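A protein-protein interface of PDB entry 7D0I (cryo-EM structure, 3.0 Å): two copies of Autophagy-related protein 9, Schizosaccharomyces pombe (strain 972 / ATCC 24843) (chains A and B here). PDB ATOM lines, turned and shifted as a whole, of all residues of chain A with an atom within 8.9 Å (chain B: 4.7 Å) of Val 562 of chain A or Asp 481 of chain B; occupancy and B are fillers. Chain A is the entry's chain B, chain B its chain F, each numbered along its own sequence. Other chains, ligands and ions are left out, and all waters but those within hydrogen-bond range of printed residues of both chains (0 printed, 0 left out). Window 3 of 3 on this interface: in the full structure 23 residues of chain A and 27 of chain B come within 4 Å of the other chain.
The side-chain carboxylate (OD2) of Asp 558 of chain A is in hydrogen-bond range of the side-chain hydroxyl (OG1) of Thr 560 of chain A (3.3 Å).
Printed residues of chain B that touch a printed residue of chain A: Glu 477, Asn 480, Asp 481 and Tyr 483.
Among the printed residues, merely in contact across the chains: Thr 560 of chain A with Tyr 483 of chain B (3.4 Å), Val 562 of chain A with Asn 480 of chain B (3.7 Å), Thr 560 of chain A with Asn 480 of chain B (3.8 Å), Val 562 of chain A with Asp 481 of chain B (3.9 Å) and Val 562 of chain A with Glu 477 of chain B (3.9 Å).
No position is printed for both chains. Of the 5 pairs that touch across the chains among the printed residues, none has its exchanged pair printed and touching as well.
Val 562 of chain A touches just these residues of chain B: Glu 477, Asn 480 and Asp 481. Of the printed residues of chain A, Asp 481 of chain B touches Val 562 (3.9 Å). Ser 482 of chain B touches none of the printed residues of chain A. Of the printed residues of chain A, Glu 477 of chain B touches Val 562. Of the printed residues of chain A, Asn 480 of chain B touches Thr 560 (3.8 Å) and Val 562 (3.7 Å). The nearest residue of chain A that does not touch Asp 481 of chain B is Thr 560 of chain A (5.6 Å).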
ATOM      1  N   HIS A 488      20.963   5.101 -25.702  1.00  0.00           N
ATOM      2  CA  HIS A 488      19.659   5.638 -25.352  1.00  0.00           C
ATOM      3  C   HIS A 488      19.776   7.069 -24.851  1.00  0.00           C
ATOM      4  O   HIS A 488      19.030   7.950 -25.282  1.00  0.00           O
ATOM      5  CB  HIS A 488      19.003   4.753 -24.303  1.00  0.00           C
ATOM      6  CG  HIS A 488      17.614   5.169 -23.950  1.00  0.00           C
ATOM      7  ND1 HIS A 488      16.707   5.597 -24.891  1.00  0.00           N
ATOM      8  CD2 HIS A 488      16.973   5.213 -22.759  1.00  0.00           C
ATOM      9  CE1 HIS A 488      15.567   5.893 -24.297  1.00  0.00           C
ATOM     10  NE2 HIS A 488      15.703   5.670 -23.003  1.00  0.00           N
ATOM     11  N   SER A 491      20.290  10.147 -27.178  1.00  0.00           N
ATOM     12  CA  SER A 491      19.199  10.412 -28.100  1.00  0.00           C
ATOM     13  C   SER A 491      18.047  11.174 -27.464  1.00  0.00           C
ATOM     14  O   SER A 491      17.094  11.522 -28.162  1.00  0.00           O
ATOM     15  CB  SER A 491      18.673   9.103 -28.684  1.00  0.00           C
ATOM     16  OG  SER A 491      17.905   8.408 -27.725  1.00  0.00           O
ATOM     17  N   GLN A 492      18.108  11.448 -26.168  1.00  0.00           N
ATOM     18  CA  GLN A 492      17.027  12.122 -25.467  1.00  0.00           C
ATOM     19  C   GLN A 492      17.057  13.627 -25.636  1.00  0.00           C
ATOM     20  O   GLN A 492      16.358  14.321 -24.896  1.00  0.00           O
ATOM     21  CB  GLN A 492      17.071  11.790 -23.979  1.00  0.00           C
ATOM     22  CG  GLN A 492      17.072  10.320 -23.672  1.00  0.00           C
ATOM     23  CD  GLN A 492      15.805   9.645 -24.093  1.00  0.00           C
ATOM     24  OE1 GLN A 492      14.849   9.582 -23.334  1.00  0.00           O
ATOM     25  NE2 GLN A 492      15.789   9.125 -25.307  1.00  0.00           N
ATOM     26  N   PRO A 494      16.375  15.909 -28.573  1.00  0.00           N
ATOM     27  CA  PRO A 494      15.986  16.257 -29.939  1.00  0.00           C
ATOM     28  C   PRO A 494      15.895  17.767 -30.109  1.00  0.00           C
ATOM     29  O   PRO A 494      15.905  18.534 -29.148  1.00  0.00           O
ATOM     30  CB  PRO A 494      14.615  15.597 -30.075  1.00  0.00           C
ATOM     31  CG  PRO A 494      14.057  15.678 -28.714  1.00  0.00           C
ATOM     32  CD  PRO A 494      15.208  15.538 -27.759  1.00  0.00           C
ATOM     33  N   PHE A 496      13.508  20.415 -31.147  1.00  0.00           N
ATOM     34  CA  PHE A 496      12.081  20.597 -31.376  1.00  0.00           C
ATOM     35  C   PHE A 496      11.814  21.644 -32.450  1.00  0.00           C
ATOM     36  O   PHE A 496      10.893  21.485 -33.259  1.00  0.00           O
ATOM     37  CB  PHE A 496      11.390  20.972 -30.071  1.00  0.00           C
ATOM     38  CG  PHE A 496      11.411  19.883 -29.052  1.00  0.00           C
ATOM     39  CD1 PHE A 496      10.776  18.681 -29.298  1.00  0.00           C
ATOM     40  CD2 PHE A 496      12.055  20.058 -27.845  1.00  0.00           C
ATOM     41  CE1 PHE A 496      10.791  17.673 -28.364  1.00  0.00           C
ATOM     42  CE2 PHE A 496      12.073  19.053 -26.905  1.00  0.00           C
ATOM     43  CZ  PHE A 496      11.439  17.859 -27.165  1.00  0.00           C
ATOM     44  N   PRO A 557      10.303  12.176 -34.592  1.00  0.00           N
ATOM     45  CA  PRO A 557      10.157  11.030 -33.696  1.00  0.00           C
ATOM     46  C   PRO A 557       8.710  10.570 -33.632  1.00  0.00           C
ATOM     47  O   PRO A 557       7.797  11.199 -34.166  1.00  0.00           O
ATOM     48  CB  PRO A 557      10.632  11.577 -32.350  1.00  0.00           C
ATOM     49  CG  PRO A 557      10.346  13.022 -32.427  1.00  0.00           C
ATOM     50  CD  PRO A 557      10.572  13.417 -33.853  1.00  0.00           C
ATOM     51  N   ASP A 558       8.514   9.439 -32.969  1.00  0.00           N
ATOM     52  CA  ASP A 558       7.167   8.940 -32.754  1.00  0.00           C
ATOM     53  C   ASP A 558       6.395   9.902 -31.864  1.00  0.00           C
ATOM     54  O   ASP A 558       6.973  10.646 -31.069  1.00  0.00           O
ATOM     55  CB  ASP A 558       7.212   7.552 -32.123  1.00  0.00           C
ATOM     56  CG  ASP A 558       5.849   6.905 -32.035  1.00  0.00           C
ATOM     57  OD1 ASP A 558       4.903   7.410 -32.674  1.00  0.00           O
ATOM     58  OD2 ASP A 558       5.722   5.892 -31.321  1.00  0.00           O
ATOM     59  N   GLU A 559       5.073   9.898 -32.015  1.00  0.00           N
ATOM     60  CA  GLU A 559       4.242  10.727 -31.151  1.00  0.00           C
ATOM     61  C   GLU A 559       4.300  10.239 -29.713  1.00  0.00           C
ATOM     62  O   GLU A 559       4.574  11.016 -28.791  1.00  0.00           O
ATOM     63  CB  GLU A 559       2.797  10.727 -31.645  1.00  0.00           C
ATOM     64  CG  GLU A 559       2.575  11.431 -32.958  1.00  0.00           C
ATOM     65  CD  GLU A 559       1.109  11.545 -33.287  1.00  0.00           C
ATOM     66  OE1 GLU A 559       0.761  12.279 -34.235  1.00  0.00           O
ATOM     67  OE2 GLU A 559       0.300  10.902 -32.590  1.00  0.00           O
ATOM     68  N   THR A 560       4.058   8.950 -29.503  1.00  0.00           N
ATOM     69  CA  THR A 560       4.004   8.388 -28.163  1.00  0.00           C
ATOM     70  C   THR A 560       5.394   8.058 -27.645  1.00  0.00           C
ATOM     71  O   THR A 560       5.634   6.948 -27.162  1.00  0.00           O
ATOM     72  CB  THR A 560       3.140   7.134 -28.165  1.00  0.00           C
ATOM     73  OG1 THR A 560       3.933   6.018 -28.577  1.00  0.00           O
ATOM     74  CG2 THR A 560       2.017   7.299 -29.144  1.00  0.00           C
ATOM     75  N   LEU A 561       6.308   9.016 -27.726  1.00  0.00           N
ATOM     76  CA  LEU A 561       7.679   8.841 -27.271  1.00  0.00           C
ATOM     77  C   LEU A 561       7.945   9.852 -26.170  1.00  0.00           C
ATOM     78  O   LEU A 561       7.716  11.049 -26.357  1.00  0.00           O
ATOM     79  CB  LEU A 561       8.667   9.026 -28.419  1.00  0.00           C
ATOM     80  CG  LEU A 561       9.935   8.177 -28.418  1.00  0.00           C
ATOM     81  CD1 LEU A 561       9.577   6.716 -28.495  1.00  0.00           C
ATOM     82  CD2 LEU A 561      10.814   8.559 -29.583  1.00  0.00           C
ATOM     83  N   VAL A 562       8.413   9.371 -25.029  1.00  0.00           N
ATOM     84  CA  VAL A 562       8.624  10.200 -23.850  1.00  0.00           C
ATOM     85  C   VAL A 562      10.122  10.388 -23.681  1.00  0.00           C
ATOM     86  O   VAL A 562      10.854   9.425 -23.421  1.00  0.00           O
ATOM     87  CB  VAL A 562       7.993   9.581 -22.598  1.00  0.00           C
ATOM     88  CG1 VAL A 562       8.233  10.472 -21.399  1.00  0.00           C
ATOM     89  CG2 VAL A 562       6.509   9.361 -22.813  1.00  0.00           C
ATOM     90  N   PHE A 563      10.579  11.626 -23.826  1.00  0.00           N
ATOM     91  CA  PHE A 563      11.982  11.964 -23.651  1.00  0.00           C
ATOM     92  C   PHE A 563      12.241  12.308 -22.194  1.00  0.00           C
ATOM     93  O   PHE A 563      11.580  13.184 -21.631  1.00  0.00           O
ATOM     94  CB  PHE A 563      12.361  13.137 -24.548  1.00  0.00           C
ATOM     95  CG  PHE A 563      12.230  12.842 -26.001  1.00  0.00           C
ATOM     96  CD1 PHE A 563      12.789  11.703 -26.535  1.00  0.00           C
ATOM     97  CD2 PHE A 563      11.536  13.690 -26.833  1.00  0.00           C
ATOM     98  CE1 PHE A 563      12.672  11.424 -27.873  1.00  0.00           C
ATOM     99  CE2 PHE A 563      11.415  13.411 -28.170  1.00  0.00           C
ATOM    100  CZ  PHE A 563      11.983  12.275 -28.690  1.00  0.00           C
ATOM    101  N   ALA A 564      13.201  11.618 -21.587  1.00  0.00           N
ATOM    102  CA  ALA A 564      13.555  11.846 -20.188  1.00  0.00           C
ATOM    103  C   ALA A 564      15.056  11.696 -20.042  1.00  0.00           C
ATOM    104  O   ALA A 564      15.562  10.609 -19.732  1.00  0.00           O
ATOM    105  CB  ALA A 564      12.814  10.881 -19.263  1.00  0.00           C
ATOM    106  N   PRO A 565      15.810  12.773 -20.258  1.00  0.00           N
ATOM    107  CA  PRO A 565      17.272  12.659 -20.207  1.00  0.00           C
ATOM    108  C   PRO A 565      17.824  12.315 -18.836  1.00  0.00           C
ATOM    109  O   PRO A 565      18.853  11.638 -18.759  1.00  0.00           O
ATOM    110  CB  PRO A 565      17.744  14.038 -20.674  1.00  0.00           C
ATOM    111  CG  PRO A 565      16.593  14.928 -20.476  1.00  0.00           C
ATOM    112  CD  PRO A 565      15.383  14.102 -20.711  1.00  0.00           C
ATOM    113  N   LYS A 567      16.658  10.362 -16.283  1.00  0.00           N
ATOM    114  CA  LYS A 567      16.642   8.958 -15.892  1.00  0.00           C
ATOM    115  C   LYS A 567      17.447   8.097 -16.852  1.00  0.00           C
ATOM    116  O   LYS A 567      17.997   7.075 -16.438  1.00  0.00           O
ATOM    117  CB  LYS A 567      15.209   8.443 -15.773  1.00  0.00           C
ATOM    118  CG  LYS A 567      14.360   8.644 -16.992  1.00  0.00           C
ATOM    119  CD  LYS A 567      12.978   8.054 -16.783  1.00  0.00           C
ATOM    120  CE  LYS A 567      13.040   6.544 -16.612  1.00  0.00           C
ATOM    121  NZ  LYS A 567      13.581   5.862 -17.822  1.00  0.00           N
ATOM    122  N   ALA A 568      17.569   8.508 -18.112  1.00  0.00           N
ATOM    123  CA  ALA A 568      18.516   7.850 -19.004  1.00  0.00           C
ATOM    124  C   ALA A 568      19.940   8.022 -18.503  1.00  0.00           C
ATOM    125  O   ALA A 568      20.733   7.072 -18.509  1.00  0.00           O
ATOM    126  CB  ALA A 568      18.378   8.403 -20.419  1.00  0.00           C
ATOM    127  N   GLU B 477       2.830  11.948 -20.227  1.00  0.00           N
ATOM    128  CA  GLU B 477       3.848  10.921 -20.039  1.00  0.00           C
ATOM    129  C   GLU B 477       3.217   9.578 -19.728  1.00  0.00           C
ATOM    130  O   GLU B 477       3.534   8.570 -20.364  1.00  0.00           O
ATOM    131  CB  GLU B 477       4.806  11.311 -18.920  1.00  0.00           C
ATOM    132  CG  GLU B 477       5.661  12.525 -19.203  1.00  0.00           C
ATOM    133  CD  GLU B 477       6.500  12.920 -18.008  1.00  0.00           C
ATOM    134  OE1 GLU B 477       6.514  12.161 -17.018  1.00  0.00           O
ATOM    135  OE2 GLU B 477       7.137  13.990 -18.057  1.00  0.00           O
ATOM    136  N   ARG B 478       2.319   9.538 -18.749  1.00  0.00           N
ATOM    137  CA  ARG B 478       1.777   8.251 -18.339  1.00  0.00           C
ATOM    138  C   ARG B 478       0.741   7.702 -19.302  1.00  0.00           C
ATOM    139  O   ARG B 478       0.396   6.525 -19.199  1.00  0.00           O
ATOM    140  CB  ARG B 478       1.178   8.338 -16.941  1.00  0.00           C
ATOM    141  CG  ARG B 478      -0.301   8.564 -16.892  1.00  0.00           C
ATOM    142  CD  ARG B 478      -0.823   8.200 -15.534  1.00  0.00           C
ATOM    143  NE  ARG B 478      -1.960   9.016 -15.149  1.00  0.00           N
ATOM    144  CZ  ARG B 478      -3.212   8.724 -15.453  1.00  0.00           C
ATOM    145  NH1 ARG B 478      -3.483   7.641 -16.150  1.00  0.00           N
ATOM    146  NH2 ARG B 478      -4.190   9.517 -15.064  1.00  0.00           N
ATOM    147  N   ILE B 479       0.237   8.501 -20.231  1.00  0.00           N
ATOM    148  CA  ILE B 479      -0.625   7.965 -21.274  1.00  0.00           C
ATOM    149  C   ILE B 479       0.191   7.460 -22.452  1.00  0.00           C
ATOM    150  O   ILE B 479      -0.106   6.405 -23.008  1.00  0.00           O
ATOM    151  CB  ILE B 479      -1.663   9.017 -21.707  1.00  0.00           C
ATOM    152  CG1 ILE B 479      -2.815   9.054 -20.711  1.00  0.00           C
ATOM    153  CG2 ILE B 479      -2.187   8.727 -23.081  1.00  0.00           C
ATOM    154  CD1 ILE B 479      -3.378   7.708 -20.360  1.00  0.00           C
ATOM    155  N   ASN B 480       1.239   8.183 -22.848  1.00  0.00           N
ATOM    156  CA  ASN B 480       2.126   7.676 -23.886  1.00  0.00           C
ATOM    157  C   ASN B 480       2.827   6.402 -23.447  1.00  0.00           C
ATOM    158  O   ASN B 480       3.064   5.514 -24.268  1.00  0.00           O
ATOM    159  CB  ASN B 480       3.157   8.732 -24.267  1.00  0.00           C
ATOM    160  CG  ASN B 480       2.540   9.913 -24.968  1.00  0.00           C
ATOM    161  OD1 ASN B 480       1.507   9.790 -25.617  1.00  0.00           O
ATOM    162  ND2 ASN B 480       3.172  11.068 -24.848  1.00  0.00           N
ATOM    163  N   ASP B 481       3.161   6.287 -22.170  1.00  0.00           N
ATOM    164  CA  ASP B 481       3.768   5.064 -21.673  1.00  0.00           C
ATOM    165  C   ASP B 481       2.783   3.925 -21.543  1.00  0.00           C
ATOM    166  O   ASP B 481       3.134   2.891 -20.980  1.00  0.00           O
ATOM    167  CB  ASP B 481       4.438   5.323 -20.326  1.00  0.00           C
ATOM    168  CG  ASP B 481       5.821   5.929 -20.468  1.00  0.00           C
ATOM    169  OD1 ASP B 481       6.487   5.666 -21.490  1.00  0.00           O
ATOM    170  OD2 ASP B 481       6.251   6.657 -19.551  1.00  0.00           O
ATOM    171  N   SER B 482       1.564   4.080 -22.043  1.00  0.00           N
ATOM    172  CA  SER B 482       0.540   3.055 -21.955  1.00  0.00           C
ATOM    173  C   SER B 482       0.136   2.480 -23.295  1.00  0.00           C
ATOM    174  O   SER B 482      -0.611   1.500 -23.323  1.00  0.00           O
ATOM    175  CB  SER B 482      -0.715   3.613 -21.280  1.00  0.00           C
ATOM    176  OG  SER B 482      -1.869   3.043 -21.854  1.00  0.00           O
ATOM    177  N   TYR B 483       0.587   3.065 -24.400  1.00  0.00           N
ATOM    178  CA  TYR B 483       0.162   2.580 -25.703  1.00  0.00           C
ATOM    179  C   TYR B 483       0.771   1.230 -26.026  1.00  0.00           C
ATOM    180  O   TYR B 483       0.139   0.420 -26.709  1.00  0.00           O
ATOM    181  CB  TYR B 483       0.515   3.593 -26.780  1.00  0.00           C
ATOM    182  CG  TYR B 483      -0.434   4.752 -26.854  1.00  0.00           C
ATOM    183  CD1 TYR B 483      -1.773   4.553 -27.092  1.00  0.00           C
ATOM    184  CD2 TYR B 483       0.012   6.045 -26.703  1.00  0.00           C
ATOM    185  CE1 TYR B 483      -2.636   5.600 -27.167  1.00  0.00           C
ATOM    186  CE2 TYR B 483      -0.847   7.096 -26.780  1.00  0.00           C
ATOM    187  CZ  TYR B 483      -2.171   6.870 -27.008  1.00  0.00           C
ATOM    188  OH  TYR B 483      -3.038   7.927 -27.083  1.00  0.00           O
ATOM    189  N   PHE B 575      -1.184   1.905 -15.886  1.00  0.00           N
ATOM    190  CA  PHE B 575      -0.953   3.200 -16.510  1.00  0.00           C
ATOM    191  C   PHE B 575      -2.216   4.036 -16.599  1.00  0.00           C
ATOM    192  O   PHE B 575      -2.207   5.211 -16.237  1.00  0.00           O
ATOM    193  CB  PHE B 575      -0.384   3.029 -17.916  1.00  0.00           C
ATOM    194  CG  PHE B 575       0.931   2.334 -17.968  1.00  0.00           C
ATOM    195  CD1 PHE B 575       2.093   3.007 -17.681  1.00  0.00           C
ATOM    196  CD2 PHE B 575       1.009   1.012 -18.343  1.00  0.00           C
ATOM    197  CE1 PHE B 575       3.299   2.365 -17.743  1.00  0.00           C
ATOM    198  CE2 PHE B 575       2.210   0.374 -18.407  1.00  0.00           C
ATOM    199  CZ  PHE B 575       3.355   1.049 -18.107  1.00  0.00           C
